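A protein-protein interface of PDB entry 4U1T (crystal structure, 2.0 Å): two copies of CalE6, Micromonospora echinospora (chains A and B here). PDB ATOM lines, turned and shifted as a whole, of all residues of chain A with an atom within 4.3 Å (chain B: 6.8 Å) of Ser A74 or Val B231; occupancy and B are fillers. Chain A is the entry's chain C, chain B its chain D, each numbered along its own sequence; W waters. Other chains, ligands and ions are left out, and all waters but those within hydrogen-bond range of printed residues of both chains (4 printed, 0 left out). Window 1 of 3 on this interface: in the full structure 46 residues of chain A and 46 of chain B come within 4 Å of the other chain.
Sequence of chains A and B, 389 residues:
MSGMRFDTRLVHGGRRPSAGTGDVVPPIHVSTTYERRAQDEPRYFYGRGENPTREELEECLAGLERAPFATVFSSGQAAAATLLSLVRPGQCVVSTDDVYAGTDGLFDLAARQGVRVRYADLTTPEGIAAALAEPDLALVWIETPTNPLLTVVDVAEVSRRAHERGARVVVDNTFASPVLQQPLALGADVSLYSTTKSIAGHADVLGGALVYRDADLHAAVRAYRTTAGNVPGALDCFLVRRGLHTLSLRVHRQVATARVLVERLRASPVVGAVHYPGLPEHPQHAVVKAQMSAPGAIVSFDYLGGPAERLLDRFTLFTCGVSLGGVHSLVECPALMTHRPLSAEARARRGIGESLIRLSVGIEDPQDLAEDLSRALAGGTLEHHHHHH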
ATOM      1  N   PHE A  73     -23.885   8.268  -4.423  1.00  0.00           N
ATOM      2  CA  PHE A  73     -23.544   9.285  -3.440  1.00  0.00           C
ATOM      3  C   PHE A  73     -22.065   9.255  -3.110  1.00  0.00           C
ATOM      4  O   PHE A  73     -21.382   8.284  -3.406  1.00  0.00           O
ATOM      5  CB  PHE A  73     -24.336   9.071  -2.146  1.00  0.00           C
ATOM      6  CG  PHE A  73     -25.818   9.204  -2.316  1.00  0.00           C
ATOM      7  CD1 PHE A  73     -26.580   8.125  -2.738  1.00  0.00           C
ATOM      8  CD2 PHE A  73     -26.444  10.426  -2.105  1.00  0.00           C
ATOM      9  CE1 PHE A  73     -27.952   8.246  -2.902  1.00  0.00           C
ATOM     10  CE2 PHE A  73     -27.829  10.559  -2.277  1.00  0.00           C
ATOM     11  CZ  PHE A  73     -28.577   9.461  -2.677  1.00  0.00           C
ATOM     12  N   SER A  74     -21.600  10.302  -2.439  1.00  0.00           N
ATOM     13  CA  SER A  74     -20.208  10.423  -2.025  1.00  0.00           C
ATOM     14  C   SER A  74     -19.760   9.321  -1.061  1.00  0.00           C
ATOM     15  O   SER A  74     -18.563   9.078  -0.943  1.00  0.00           O
ATOM     16  CB  SER A  74     -19.988  11.806  -1.382  1.00  0.00           C
ATOM     17  OG  SER A  74     -20.982  12.039  -0.383  1.00  0.00           O
ATOM     18  N   SER A  75     -20.714   8.664  -0.391  1.00  0.00           N
ATOM     19  CA  SER A  75     -20.446   7.561   0.539  1.00  0.00           C
ATOM     20  C   SER A  75     -21.737   6.792   0.884  1.00  0.00           C
ATOM     21  O   SER A  75     -22.841   7.266   0.602  1.00  0.00           O
ATOM     22  CB  SER A  75     -19.806   8.080   1.825  1.00  0.00           C
ATOM     23  OG  SER A  75     -20.731   8.886   2.568  1.00  0.00           O
ATOM     24  N   ALA A  78     -23.825   8.847   3.166  1.00  0.00           N
ATOM     25  CA  ALA A  78     -24.579   9.882   2.451  1.00  0.00           C
ATOM     26  C   ALA A  78     -25.855   9.323   1.838  1.00  0.00           C
ATOM     27  O   ALA A  78     -26.888  10.006   1.806  1.00  0.00           O
ATOM     28  CB  ALA A  78     -23.713  10.545   1.360  1.00  0.00           C
ATOM     29  N   LEU A 206     -14.446   5.730  -2.064  1.00  0.00           N
ATOM     30  CA  LEU A 206     -15.649   5.808  -1.223  1.00  0.00           C
ATOM     31  C   LEU A 206     -16.858   6.011  -2.112  1.00  0.00           C
ATOM     32  O   LEU A 206     -16.769   6.705  -3.123  1.00  0.00           O
ATOM     33  CB  LEU A 206     -15.545   6.970  -0.227  1.00  0.00           C
ATOM     34  CG  LEU A 206     -14.396   7.004   0.786  1.00  0.00           C
ATOM     35  CD1 LEU A 206     -14.410   8.334   1.572  1.00  0.00           C
ATOM     36  CD2 LEU A 206     -14.429   5.805   1.741  1.00  0.00           C
ATOM     37  N   GLY A 207     -17.989   5.413  -1.760  1.00  0.00           N
ATOM     38  CA  GLY A 207     -19.205   5.687  -2.509  1.00  0.00           C
ATOM     39  C   GLY A 207     -20.411   5.065  -1.836  1.00  0.00           C
ATOM     40  O   GLY A 207     -20.272   4.189  -0.987  1.00  0.00           O
ATOM     41  N   ASN A 230     -24.286  15.972  -1.733  1.00  0.00           N
ATOM     42  CA  ASN A 230     -23.497  14.801  -1.345  1.00  0.00           C
ATOM     43  C   ASN A 230     -23.260  13.867  -2.543  1.00  0.00           C
ATOM     44  O   ASN A 230     -23.490  12.650  -2.491  1.00  0.00           O
ATOM     45  CB  ASN A 230     -24.170  14.068  -0.164  1.00  0.00           C
ATOM     46  CG  ASN A 230     -25.642  13.777  -0.405  1.00  0.00           C
ATOM     47  OD1 ASN A 230     -26.179  14.044  -1.479  1.00  0.00           O
ATOM     48  ND2 ASN A 230     -26.295  13.187   0.596  1.00  0.00           N
ATOM     49  N   VAL A 231     -22.768  14.465  -3.629  1.00  0.00           N
ATOM     50  CA  VAL A 231     -22.525  13.757  -4.883  1.00  0.00           C
ATOM     51  C   VAL A 231     -21.092  13.225  -4.974  1.00  0.00           C
ATOM     52  O   VAL A 231     -20.160  13.857  -4.482  1.00  0.00           O
ATOM     53  CB  VAL A 231     -22.783  14.676  -6.100  1.00  0.00           C
ATOM     54  CG1 VAL A 231     -24.259  14.978  -6.218  1.00  0.00           C
ATOM     55  CG2 VAL A 231     -22.010  15.974  -5.960  1.00  0.00           C
ATOM     56  N   PRO A 232     -20.910  12.071  -5.624  1.00  0.00           N
ATOM     57  CA  PRO A 232     -19.553  11.541  -5.832  1.00  0.00           C
ATOM     58  C   PRO A 232     -18.841  12.236  -7.005  1.00  0.00           C
ATOM     59  O   PRO A 232     -19.509  12.807  -7.859  1.00  0.00           O
ATOM     60  CB  PRO A 232     -19.811  10.067  -6.139  1.00  0.00           C
ATOM     61  CG  PRO A 232     -21.140  10.070  -6.850  1.00  0.00           C
ATOM     62  CD  PRO A 232     -21.947  11.200  -6.214  1.00  0.00           C
ATOM     63  N   GLY B  47     -11.129   5.859   5.556  1.00  0.00           N
ATOM     64  CA  GLY B  47     -11.058   6.978   4.632  1.00  0.00           C
ATOM     65  C   GLY B  47     -12.132   8.040   4.777  1.00  0.00           C
ATOM     66  O   GLY B  47     -11.876   9.213   4.510  1.00  0.00           O
ATOM     67  N   ARG B  48     -13.337   7.653   5.187  1.00  0.00           N
ATOM     68  CA  ARG B  48     -14.380   8.657   5.374  1.00  0.00           C
ATOM     69  C   ARG B  48     -13.987   9.592   6.533  1.00  0.00           C
ATOM     70  O   ARG B  48     -14.245  10.801   6.496  1.00  0.00           O
ATOM     71  CB  ARG B  48     -15.752   8.004   5.617  1.00  0.00           C
ATOM     72  CG  ARG B  48     -16.844   9.016   5.963  1.00  0.00           C
ATOM     73  CD  ARG B  48     -18.270   8.519   5.696  1.00  0.00           C
ATOM     74  NE  ARG B  48     -18.452   7.100   5.980  1.00  0.00           N
ATOM     75  CZ  ARG B  48     -18.538   6.588   7.203  1.00  0.00           C
ATOM     76  NH1 ARG B  48     -18.468   7.384   8.264  1.00  0.00           N
ATOM     77  NH2 ARG B  48     -18.704   5.280   7.368  1.00  0.00           N
ATOM     78  N   GLY B  49     -13.340   9.036   7.555  1.00  0.00           N
ATOM     79  CA  GLY B  49     -12.908   9.833   8.694  1.00  0.00           C
ATOM     80  C   GLY B  49     -11.572  10.537   8.487  1.00  0.00           C
ATOM     81  O   GLY B  49     -11.414  11.712   8.835  1.00  0.00           O
ATOM     82  N   ARG B  54      -6.628  14.641   1.600  1.00  0.00           N
ATOM     83  CA  ARG B  54      -7.665  15.579   1.991  1.00  0.00           C
ATOM     84  C   ARG B  54      -7.139  16.554   3.055  1.00  0.00           C
ATOM     85  O   ARG B  54      -7.350  17.779   2.982  1.00  0.00           O
ATOM     86  CB  ARG B  54      -8.878  14.794   2.499  1.00  0.00           C
ATOM     87  CG  ARG B  54     -10.096  15.617   2.772  1.00  0.00           C
ATOM     88  CD  ARG B  54     -11.319  14.722   3.010  1.00  0.00           C
ATOM     89  NE  ARG B  54     -11.250  14.022   4.285  1.00  0.00           N
ATOM     90  CZ  ARG B  54     -11.514  12.723   4.454  1.00  0.00           C
ATOM     91  NH1 ARG B  54     -11.827  11.962   3.418  1.00  0.00           N
ATOM     92  NH2 ARG B  54     -11.453  12.185   5.664  1.00  0.00           N
ATOM     93  N   VAL B  72     -12.922  20.245   4.034  1.00  0.00           N
ATOM     94  CA  VAL B  72     -13.409  20.181   2.654  1.00  0.00           C
ATOM     95  C   VAL B  72     -14.524  19.151   2.503  1.00  0.00           C
ATOM     96  O   VAL B  72     -14.659  18.220   3.308  1.00  0.00           O
ATOM     97  CB  VAL B  72     -12.271  19.859   1.656  1.00  0.00           C
ATOM     98  CG1 VAL B  72     -11.248  20.993   1.636  1.00  0.00           C
ATOM     99  CG2 VAL B  72     -11.598  18.529   2.024  1.00  0.00           C
ATOM    100  N   PHE B  73     -15.303  19.332   1.445  1.00  0.00           N
ATOM    101  CA  PHE B  73     -16.541  18.617   1.240  1.00  0.00           C
ATOM    102  C   PHE B  73     -16.708  18.210  -0.212  1.00  0.00           C
ATOM    103  O   PHE B  73     -16.028  18.730  -1.087  1.00  0.00           O
ATOM    104  CB  PHE B  73     -17.742  19.480   1.644  1.00  0.00           C
ATOM    105  CG  PHE B  73     -17.765  19.848   3.093  1.00  0.00           C
ATOM    106  CD1 PHE B  73     -17.028  20.923   3.567  1.00  0.00           C
ATOM    107  CD2 PHE B  73     -18.486  19.078   3.993  1.00  0.00           C
ATOM    108  CE1 PHE B  73     -17.057  21.256   4.920  1.00  0.00           C
ATOM    109  CE2 PHE B  73     -18.505  19.391   5.347  1.00  0.00           C
ATOM    110  CZ  PHE B  73     -17.792  20.482   5.804  1.00  0.00           C
ATOM    111  N   SER B  74     -17.666  17.331  -0.462  1.00  0.00           N
ATOM    112  CA  SER B  74     -17.960  16.867  -1.814  1.00  0.00           C
ATOM    113  C   SER B  74     -18.416  17.985  -2.759  1.00  0.00           C
ATOM    114  O   SER B  74     -18.314  17.839  -3.974  1.00  0.00           O
ATOM    115  CB  SER B  74     -19.038  15.770  -1.739  1.00  0.00           C
ATOM    116  OG  SER B  74     -20.133  16.222  -0.955  1.00  0.00           O
ATOM    117  N   SER B  75     -18.918  19.099  -2.208  1.00  0.00           N
ATOM    118  CA  SER B  75     -19.338  20.247  -3.020  1.00  0.00           C
ATOM    119  C   SER B  75     -19.510  21.483  -2.156  1.00  0.00           C
ATOM    120  O   SER B  75     -19.504  21.389  -0.928  1.00  0.00           O
ATOM    121  CB  SER B  75     -20.659  19.966  -3.759  1.00  0.00           C
ATOM    122  OG  SER B  75     -21.729  19.843  -2.825  1.00  0.00           O
ATOM    123  N   ALA B  78     -22.576  21.066  -0.056  1.00  0.00           N
ATOM    124  CA  ALA B  78     -22.374  20.229   1.129  1.00  0.00           C
ATOM    125  C   ALA B  78     -21.709  21.002   2.267  1.00  0.00           C
ATOM    126  O   ALA B  78     -22.025  20.805   3.451  1.00  0.00           O
ATOM    127  CB  ALA B  78     -21.543  18.983   0.758  1.00  0.00           C
ATOM    128  N   ARG B 225     -19.653  15.978   9.078  1.00  0.00           N
ATOM    129  CA  ARG B 225     -19.142  15.471   7.805  1.00  0.00           C
ATOM    130  C   ARG B 225     -18.983  13.945   7.844  1.00  0.00           C
ATOM    131  O   ARG B 225     -19.282  13.257   6.884  1.00  0.00           O
ATOM    132  CB  ARG B 225     -17.799  16.121   7.426  1.00  0.00           C
ATOM    133  CG  ARG B 225     -17.338  15.733   6.019  1.00  0.00           C
ATOM    134  CD  ARG B 225     -15.958  16.302   5.645  1.00  0.00           C
ATOM    135  NE  ARG B 225     -14.915  15.755   6.504  1.00  0.00           N
ATOM    136  CZ  ARG B 225     -13.617  16.012   6.384  1.00  0.00           C
ATOM    137  NH1 ARG B 225     -13.167  16.827   5.425  1.00  0.00           N
ATOM    138  NH2 ARG B 225     -12.772  15.460   7.240  1.00  0.00           N
ATOM    139  N   THR B 226     -18.508  13.431   8.964  1.00  0.00           N
ATOM    140  CA  THR B 226     -18.314  11.991   9.132  1.00  0.00           C
ATOM    141  C   THR B 226     -19.643  11.237   9.141  1.00  0.00           C
ATOM    142  O   THR B 226     -19.771  10.186   8.528  1.00  0.00           O
ATOM    143  CB  THR B 226     -17.556  11.705  10.436  1.00  0.00           C
ATOM    144  OG1 THR B 226     -16.273  12.336  10.369  1.00  0.00           O
ATOM    145  CG2 THR B 226     -17.367  10.203  10.655  1.00  0.00           C
ATOM    146  N   ALA B 228     -22.783  12.496   8.069  1.00  0.00           N
ATOM    147  CA  ALA B 228     -23.496  12.720   6.811  1.00  0.00           C
ATOM    148  C   ALA B 228     -22.754  12.129   5.599  1.00  0.00           C
ATOM    149  O   ALA B 228     -23.360  11.863   4.561  1.00  0.00           O
ATOM    150  CB  ALA B 228     -23.740  14.195   6.599  1.00  0.00           C
ATOM    151  N   GLY B 229     -21.449  11.936   5.724  1.00  0.00           N
ATOM    152  CA  GLY B 229     -20.683  11.294   4.668  1.00  0.00           C
ATOM    153  C   GLY B 229     -20.518  12.138   3.406  1.00  0.00           C
ATOM    154  O   GLY B 229     -20.327  11.595   2.317  1.00  0.00           O
ATOM    155  N   ASN B 230     -20.588  13.460   3.547  1.00  0.00           N
ATOM    156  CA  ASN B 230     -20.428  14.350   2.394  1.00  0.00           C
ATOM    157  C   ASN B 230     -18.951  14.745   2.167  1.00  0.00           C
ATOM    158  O   ASN B 230     -18.607  15.923   2.008  1.00  0.00           O
ATOM    159  CB  ASN B 230     -21.331  15.591   2.540  1.00  0.00           C
ATOM    160  CG  ASN B 230     -21.183  16.290   3.882  1.00  0.00           C
ATOM    161  OD1 ASN B 230     -20.356  15.914   4.705  1.00  0.00           O
ATOM    162  ND2 ASN B 230     -21.994  17.338   4.102  1.00  0.00           N
ATOM    163  N   VAL B 231     -18.089  13.731   2.130  1.00  0.00           N
ATOM    164  CA  VAL B 231     -16.649  13.896   1.950  1.00  0.00           C
ATOM    165  C   VAL B 231     -16.264  13.814   0.476  1.00  0.00           C
ATOM    166  O   VAL B 231     -16.889  13.096  -0.296  1.00  0.00           O
ATOM    167  CB  VAL B 231     -15.840  12.805   2.698  1.00  0.00           C
ATOM    168  CG1 VAL B 231     -15.935  12.989   4.193  1.00  0.00           C
ATOM    169  CG2 VAL B 231     -16.344  11.435   2.313  1.00  0.00           C
ATOM    170  N   PRO B 232     -15.231  14.565   0.079  1.00  0.00           N
ATOM    171  CA  PRO B 232     -14.725  14.479  -1.294  1.00  0.00           C
ATOM    172  C   PRO B 232     -13.809  13.274  -1.454  1.00  0.00           C
ATOM    173  O   PRO B 232     -13.290  12.783  -0.451  1.00  0.00           O
ATOM    174  CB  PRO B 232     -13.938  15.781  -1.458  1.00  0.00           C
ATOM    175  CG  PRO B 232     -13.393  16.039  -0.062  1.00  0.00           C
ATOM    176  CD  PRO B 232     -14.462  15.523   0.899  1.00  0.00           C
ATOM    177  N   GLY B 233     -13.614  12.802  -2.680  1.00  0.00           N
ATOM    178  CA  GLY B 233     -12.655  11.734  -2.917  1.00  0.00           C
ATOM    179  C   GLY B 233     -11.235  12.276  -2.959  1.00  0.00           C
ATOM    180  O   GLY B 233     -11.028  13.469  -3.150  1.00  0.00           O
HETATM  181  O   HOH W   1     -16.275  10.360  -1.755  1.00  0.00           O
HETATM  182  O   HOH W   2     -17.720  15.537  -5.484  1.00  0.00           O
HETATM  183  O   HOH W   3     -24.997  13.503   3.178  1.00  0.00           O
HETATM  184  O   HOH W   4     -17.471  13.241  -3.238  1.00  0.00           O
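Ser A74 touches just these residues of chain B: Gly B229 (2.8 Å), Asn B230 (3.7 Å) and Val B231 (3.5 Å).
Printed residues of chain B within 4 Å of Ser A75: Arg B48 (3.997 Å) and Gly B229 (2.8 Å).
Gly A207 touches none of the printed residues of chain B.
Val B72 touches none of the printed residues of chain A.
Of the printed residues of chain A, Asn B230 touches Ser A74.
The nearest printed residue of chain B that does not touch Ser A75 is Ala B228 (4.4 Å).
Water W3 bridges the backbone carbonyl oxygen of Ala B228 (2.7 Å) and the side-chain amide nitrogen of Asn A230 (2.9 Å).
Water W1 lies within hydrogen-bond range of O of Ser A74 and O of Val B231.
Water W2 lies within hydrogen-bond range of O of Ser B74 and O of Val A231.
Water W4 bridges the backbone carbonyl oxygen (O) of Val B231 and the backbone carbonyl oxygen (O) of Val A231.
Among the printed residues, pairs that only touch across the chains: Val A231 with Ser B74 (3.5 Å), Ser A74 with Val B231 (3.5 Å), Ser A74 with Asn B230 (3.7 Å), Ala A78 with Gly B229 (3.7 Å), Asn A230 with Ser B74 (3.7 Å), Leu A206 with Val B231 (3.7 Å), Leu A206 with Arg B48 (3.8 Å), Leu A206 with Gly B47 (3.9 Å) and Ser A75 with Arg B48 (3.997 Å).
The backbone NH (N) of Ser B74 lies within hydrogen-bond range of the backbone carbonyl oxygen (O) of Asn B230, at 3.0 Å.
The backbone NH (N) of Ser A74 is in hydrogen-bond range of the backbone carbonyl oxygen (O) of Asn A230 (3.0 Å).
The guanidinium group of Arg B54 sits at hydrogen-bond distance from the backbone carbonyl oxygen of Gly B47, at 3.0 Å.
The backbone carbonyl oxygen (O) of Arg B48 lies within hydrogen-bond range of the guanidinium group (NH2) of Arg B54 (3.2 Å).
The side-chain hydroxyl (OG) of Ser A75 sits at hydrogen-bond distance from the backbone NH (N) of Ala A78, 3.2 Å away.
The side-chain amide nitrogen (ND2) of Asn A230 sits at hydrogen-bond distance from the backbone carbonyl oxygen (O) of Ala A78 (3.5 Å).
Printed residues of chain A that touch a printed residue of chain B: Ser A74, Ser A75, Ala A78, Leu A206, Asn A230 and Val A231.
Hydrophobic or aromatic side chains of chain A within 4 Å of the printed part of chain B: Ala A78 and Leu A206.
Among the printed residues, 12 pairs touch across the chains.
Among the printed residues, no Asp or Glu carboxylate lies within 4 Å of a Lys or Arg side-chain nitrogen of the other chain.
Ser A74 touches Asn B230, and with the chains exchanged Asn A230 touches Ser B74.
Ser A74 touches Val B231, and with the chains exchanged Val A231 touches Ser B74.
7 positions are printed for both chains.
N of Ala A78 sits close to O of Ala B228, at 3.4 Å.
The side-chain hydroxyl of Ser A74 lies within hydrogen-bond range of the backbone carbonyl oxygen of Gly B229 (2.8 Å).
O of Gly B229 is in hydrogen-bond range of OG of Ser A75 (2.8 Å).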
